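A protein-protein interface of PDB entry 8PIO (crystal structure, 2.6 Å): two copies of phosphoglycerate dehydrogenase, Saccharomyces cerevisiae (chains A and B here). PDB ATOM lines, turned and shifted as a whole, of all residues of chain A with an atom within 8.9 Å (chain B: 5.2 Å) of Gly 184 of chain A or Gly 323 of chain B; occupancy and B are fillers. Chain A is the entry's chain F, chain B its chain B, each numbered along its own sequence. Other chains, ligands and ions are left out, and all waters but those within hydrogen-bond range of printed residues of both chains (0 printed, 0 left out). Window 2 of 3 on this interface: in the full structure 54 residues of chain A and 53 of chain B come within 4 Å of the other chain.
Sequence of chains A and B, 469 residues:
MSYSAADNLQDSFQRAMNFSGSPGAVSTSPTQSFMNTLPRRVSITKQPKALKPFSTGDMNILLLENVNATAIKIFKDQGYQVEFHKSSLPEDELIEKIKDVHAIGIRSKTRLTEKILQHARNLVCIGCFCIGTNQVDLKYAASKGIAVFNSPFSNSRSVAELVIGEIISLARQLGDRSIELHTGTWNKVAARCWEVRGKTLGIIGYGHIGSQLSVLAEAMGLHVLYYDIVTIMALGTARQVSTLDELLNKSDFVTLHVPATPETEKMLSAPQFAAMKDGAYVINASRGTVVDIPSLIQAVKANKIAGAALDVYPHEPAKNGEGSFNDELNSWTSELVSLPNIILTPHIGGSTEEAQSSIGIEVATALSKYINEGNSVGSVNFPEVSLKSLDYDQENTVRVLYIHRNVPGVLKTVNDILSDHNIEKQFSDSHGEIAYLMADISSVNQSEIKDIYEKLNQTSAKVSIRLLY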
ATOM      1  N   ARG A 177      21.285   8.998  -3.612  1.00  0.00           N
ATOM      2  CA  ARG A 177      21.605  10.117  -2.679  1.00  0.00           C
ATOM      3  C   ARG A 177      20.451  10.316  -1.692  1.00  0.00           C
ATOM      4  O   ARG A 177      20.714  10.415  -0.488  1.00  0.00           O
ATOM      5  CB  ARG A 177      21.849  11.414  -3.451  1.00  0.00           C
ATOM      6  CG  ARG A 177      23.142  11.440  -4.250  1.00  0.00           C
ATOM      7  CD  ARG A 177      24.356  11.246  -3.376  1.00  0.00           C
ATOM      8  NE  ARG A 177      24.707   9.850  -3.279  1.00  0.00           N
ATOM      9  CZ  ARG A 177      25.380   9.186  -4.200  1.00  0.00           C
ATOM     10  NH1 ARG A 177      25.644   7.903  -4.025  1.00  0.00           N
ATOM     11  NH2 ARG A 177      25.790   9.806  -5.298  1.00  0.00           N
ATOM     12  N   SER A 178      19.225  10.378  -2.199  1.00  0.00           N
ATOM     13  CA  SER A 178      17.999  10.683  -1.418  1.00  0.00           C
ATOM     14  C   SER A 178      17.654   9.504  -0.505  1.00  0.00           C
ATOM     15  O   SER A 178      17.162   9.742   0.614  1.00  0.00           O
ATOM     16  CB  SER A 178      16.859  11.030  -2.315  1.00  0.00           C
ATOM     17  OG  SER A 178      15.760  11.506  -1.553  1.00  0.00           O
ATOM     18  N   ILE A 179      17.902   8.285  -0.968  1.00  0.00           N
ATOM     19  CA  ILE A 179      17.674   7.028  -0.194  1.00  0.00           C
ATOM     20  C   ILE A 179      18.677   6.984   0.965  1.00  0.00           C
ATOM     21  O   ILE A 179      18.266   6.672   2.078  1.00  0.00           O
ATOM     22  CB  ILE A 179      17.765   5.789  -1.111  1.00  0.00           C
ATOM     23  CG1 ILE A 179      16.438   5.542  -1.838  1.00  0.00           C
ATOM     24  CG2 ILE A 179      18.210   4.568  -0.328  1.00  0.00           C
ATOM     25  CD1 ILE A 179      16.551   4.654  -3.055  1.00  0.00           C
ATOM     26  N   GLU A 180      19.939   7.309   0.694  1.00  0.00           N
ATOM     27  CA  GLU A 180      21.028   7.367   1.709  1.00  0.00           C
ATOM     28  C   GLU A 180      20.610   8.309   2.850  1.00  0.00           C
ATOM     29  O   GLU A 180      20.623   7.869   4.008  1.00  0.00           O
ATOM     30  CB  GLU A 180      22.334   7.847   1.076  1.00  0.00           C
ATOM     31  CG  GLU A 180      22.955   6.854   0.116  1.00  0.00           C
ATOM     32  CD  GLU A 180      24.099   7.434  -0.702  1.00  0.00           C
ATOM     33  OE1 GLU A 180      24.273   8.678  -0.677  1.00  0.00           O
ATOM     34  OE2 GLU A 180      24.813   6.655  -1.357  1.00  0.00           O
ATOM     35  N   LEU A 181      20.256   9.555   2.520  1.00  0.00           N
ATOM     36  CA  LEU A 181      19.919  10.630   3.502  1.00  0.00           C
ATOM     37  C   LEU A 181      18.670  10.250   4.293  1.00  0.00           C
ATOM     38  O   LEU A 181      18.580  10.641   5.457  1.00  0.00           O
ATOM     39  CB  LEU A 181      19.708  11.951   2.767  1.00  0.00           C
ATOM     40  CG  LEU A 181      20.907  12.888   2.757  1.00  0.00           C
ATOM     41  CD1 LEU A 181      20.628  14.106   1.907  1.00  0.00           C
ATOM     42  CD2 LEU A 181      21.281  13.309   4.171  1.00  0.00           C
ATOM     43  N   HIS A 182      17.743   9.538   3.673  1.00  0.00           N
ATOM     44  CA  HIS A 182      16.483   9.069   4.315  1.00  0.00           C
ATOM     45  C   HIS A 182      16.810   8.025   5.393  1.00  0.00           C
ATOM     46  O   HIS A 182      16.115   8.011   6.419  1.00  0.00           O
ATOM     47  CB  HIS A 182      15.491   8.569   3.262  1.00  0.00           C
ATOM     48  CG  HIS A 182      14.631   9.660   2.716  1.00  0.00           C
ATOM     49  ND1 HIS A 182      15.101  10.571   1.800  1.00  0.00           N
ATOM     50  CD2 HIS A 182      13.347  10.010   2.977  1.00  0.00           C
ATOM     51  CE1 HIS A 182      14.143  11.425   1.501  1.00  0.00           C
ATOM     52  NE2 HIS A 182      13.060  11.104   2.213  1.00  0.00           N
ATOM     53  N   THR A 183      17.839   7.203   5.160  1.00  0.00           N
ATOM     54  CA  THR A 183      18.365   6.185   6.116  1.00  0.00           C
ATOM     55  C   THR A 183      19.435   6.831   7.009  1.00  0.00           C
ATOM     56  O   THR A 183      20.036   6.113   7.810  1.00  0.00           O
ATOM     57  CB  THR A 183      18.916   4.955   5.376  1.00  0.00           C
ATOM     58  N   GLY A 184      19.661   8.140   6.849  1.00  0.00           N
ATOM     59  CA  GLY A 184      20.507   8.965   7.738  1.00  0.00           C
ATOM     60  C   GLY A 184      21.944   9.098   7.240  1.00  0.00           C
ATOM     61  O   GLY A 184      22.733   9.756   7.932  1.00  0.00           O
ATOM     62  N   THR A 185      22.269   8.510   6.082  1.00  0.00           N
ATOM     63  CA  THR A 185      23.646   8.497   5.495  1.00  0.00           C
ATOM     64  C   THR A 185      23.861   9.733   4.606  1.00  0.00           C
ATOM     65  O   THR A 185      23.009  10.002   3.737  1.00  0.00           O
ATOM     66  CB  THR A 185      23.915   7.219   4.693  1.00  0.00           C
ATOM     67  OG1 THR A 185      23.564   6.096   5.500  1.00  0.00           O
ATOM     68  CG2 THR A 185      25.360   7.101   4.255  1.00  0.00           C
ATOM     69  N   TRP A 186      24.974  10.433   4.823  1.00  0.00           N
ATOM     70  CA  TRP A 186      25.408  11.638   4.066  1.00  0.00           C
ATOM     71  C   TRP A 186      26.582  11.256   3.176  1.00  0.00           C
ATOM     72  O   TRP A 186      27.686  11.106   3.707  1.00  0.00           O
ATOM     73  CB  TRP A 186      25.780  12.770   5.035  1.00  0.00           C
ATOM     74  CG  TRP A 186      26.192  14.060   4.384  1.00  0.00           C
ATOM     75  CD1 TRP A 186      27.405  14.363   3.830  1.00  0.00           C
ATOM     76  CD2 TRP A 186      25.390  15.248   4.261  1.00  0.00           C
ATOM     77  NE1 TRP A 186      27.408  15.650   3.359  1.00  0.00           N
ATOM     78  CE2 TRP A 186      26.185  16.219   3.612  1.00  0.00           C
ATOM     79  CE3 TRP A 186      24.081  15.583   4.629  1.00  0.00           C
ATOM     80  CZ2 TRP A 186      25.707  17.496   3.322  1.00  0.00           C
ATOM     81  CZ3 TRP A 186      23.612  16.846   4.346  1.00  0.00           C
ATOM     82  CH2 TRP A 186      24.413  17.787   3.697  1.00  0.00           C
ATOM     83  N   ASN A 187      26.343  11.097   1.875  1.00  0.00           N
ATOM     84  CA  ASN A 187      27.352  10.597   0.906  1.00  0.00           C
ATOM     85  C   ASN A 187      27.468  11.580  -0.262  1.00  0.00           C
ATOM     86  O   ASN A 187      26.941  11.274  -1.357  1.00  0.00           O
ATOM     87  CB  ASN A 187      27.012   9.184   0.432  1.00  0.00           C
ATOM     88  CG  ASN A 187      28.116   8.557  -0.380  1.00  0.00           C
ATOM     89  OD1 ASN A 187      29.284   8.863  -0.179  1.00  0.00           O
ATOM     90  ND2 ASN A 187      27.754   7.681  -1.303  1.00  0.00           N
ATOM     91  N   GLY B 321      29.488  10.220   6.285  1.00  0.00           N
ATOM     92  CA  GLY B 321      29.339   9.271   7.402  1.00  0.00           C
ATOM     93  C   GLY B 321      27.958   8.650   7.453  1.00  0.00           C
ATOM     94  O   GLY B 321      27.027   9.255   6.909  1.00  0.00           O
ATOM     95  N   GLU B 322      27.837   7.519   8.155  1.00  0.00           N
ATOM     96  CA  GLU B 322      26.703   6.556   8.060  1.00  0.00           C
ATOM     97  C   GLU B 322      25.477   7.050   8.839  1.00  0.00           C
ATOM     98  O   GLU B 322      24.355   6.890   8.321  1.00  0.00           O
ATOM     99  CB  GLU B 322      27.128   5.190   8.590  1.00  0.00           C
ATOM    100  CG  GLU B 322      28.222   4.533   7.772  1.00  0.00           C
ATOM    101  CD  GLU B 322      27.757   3.946   6.453  1.00  0.00           C
ATOM    102  OE1 GLU B 322      28.604   3.767   5.558  1.00  0.00           O
ATOM    103  OE2 GLU B 322      26.544   3.664   6.324  1.00  0.00           O
ATOM    104  N   GLY B 323      25.677   7.585  10.040  1.00  0.00           N
ATOM    105  CA  GLY B 323      24.580   8.068  10.909  1.00  0.00           C
ATOM    106  C   GLY B 323      24.639   9.573  11.091  1.00  0.00           C
ATOM    107  O   GLY B 323      24.187  10.057  12.143  1.00  0.00           O
ATOM    108  N   SER B 324      25.180  10.277  10.091  1.00  0.00           N
ATOM    109  CA  SER B 324      25.544  11.721  10.143  1.00  0.00           C
ATOM    110  C   SER B 324      24.284  12.601  10.113  1.00  0.00           C
ATOM    111  O   SER B 324      24.287  13.653  10.786  1.00  0.00           O
ATOM    112  CB  SER B 324      26.469  12.076   9.015  1.00  0.00           C
ATOM    113  OG  SER B 324      27.556  11.181   8.947  1.00  0.00           O
ATOM    114  N   PHE B 325      23.265  12.190   9.352  1.00  0.00           N
ATOM    115  CA  PHE B 325      22.008  12.956   9.112  1.00  0.00           C
ATOM    116  C   PHE B 325      20.922  12.451  10.069  1.00  0.00           C
ATOM    117  O   PHE B 325      20.228  11.471   9.727  1.00  0.00           O
ATOM    118  CB  PHE B 325      21.587  12.836   7.640  1.00  0.00           C
ATOM    119  CG  PHE B 325      20.583  13.865   7.179  1.00  0.00           C
ATOM    120  CD1 PHE B 325      20.984  15.152   6.853  1.00  0.00           C
ATOM    121  CD2 PHE B 325      19.235  13.547   7.056  1.00  0.00           C
ATOM    122  CE1 PHE B 325      20.061  16.097   6.429  1.00  0.00           C
ATOM    123  CE2 PHE B 325      18.318  14.498   6.632  1.00  0.00           C
ATOM    124  CZ  PHE B 325      18.732  15.768   6.320  1.00  0.00           C
ATOM    125  N   ASN B 326      20.782  13.109  11.225  1.00  0.00           N
ATOM    126  CA  ASN B 326      19.971  12.619  12.375  1.00  0.00           C
ATOM    127  C   ASN B 326      19.438  13.803  13.190  1.00  0.00           C
ATOM    128  O   ASN B 326      19.761  14.964  12.845  1.00  0.00           O
ATOM    129  CB  ASN B 326      20.790  11.686  13.268  1.00  0.00           C
ATOM    130  CG  ASN B 326      22.098  12.309  13.703  1.00  0.00           C
ATOM    131  OD1 ASN B 326      22.111  13.387  14.287  1.00  0.00           O
ATOM    132  ND2 ASN B 326      23.204  11.644  13.415  1.00  0.00           N
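Of the 6 printed residues of chain B, 5 touch a printed residue of chain A.
Printed residues of chain B that touch a printed residue of chain A: Gly 321, Glu 322, Gly 323, Ser 324 and Phe 325.
Hydrophobic or aromatic side chains of chain A within 4 Å of the printed part of chain B: Leu 181 and Trp 186.
N of Thr 185 of chain A is in hydrogen-bond range of O of Glu 180 of chain A, 2.7 Å away.
O of Gly 321 of chain B sits at hydrogen-bond distance from OG of Ser 324 of chain B (2.9 Å).
O of Ser 324 of chain B sits at hydrogen-bond distance from ND2 of Asn 326 of chain B.
No position is printed for both chains.
Of chain B, only Glu 322 (3.3 Å), Gly 323 (3.7 Å), Ser 324 (3.3 Å) and Phe 325 (2.9 Å) come within 4 Å of Gly 184 of chain A.
Gly 323 of chain B touches just one residue of chain A: Gly 184 (3.7 Å).
Printed residues of chain A within 4 Å of Ser 324 of chain B: Gly 184 (3.3 Å).
Of the printed residues of chain A, Gly 321 of chain B touches Thr 185 and Trp 186.
Of the printed residues of chain B, Thr 185 of chain A touches Gly 321 and Glu 322.
The nearest printed residue of chain A that does not touch Gly 321 of chain B is Gly 184 of chain A (4.4 Å).
Among the printed residues, pairs that only touch across the chains: Leu 181 of chain A with Phe 325 of chain B (3.1 Å), Gly 184 of chain A with Gly 323 of chain B (3.7 Å), Thr 185 of chain A with Gly 321 of chain B (3.7 Å) and Trp 186 of chain A with Phe 325 of chain B (3.8 Å).
The backbone carbonyl oxygen (O) of Gly 184 of chain A is in hydrogen-bond range of the backbone NH (N) of Ser 324 of chain B (3.3 Å).
The backbone carbonyl oxygen of Gly 184 of chain A lies within hydrogen-bond range of the backbone NH of Phe 325 of chain B (2.9 Å).
The side-chain hydroxyl of Thr 185 of chain A sits at hydrogen-bond distance from the backbone carbonyl oxygen of Glu 322 of chain B (3.0 Å).
The backbone NH (N) of Trp 186 of chain A sits at hydrogen-bond distance from the backbone carbonyl oxygen (O) of Gly 321 of chain B, at 3.2 Å.
The backbone carbonyl oxygen of Glu 322 of chain B lies close to the backbone carbonyl oxygen of Gly 184 of chain A, at 3.3 Å.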
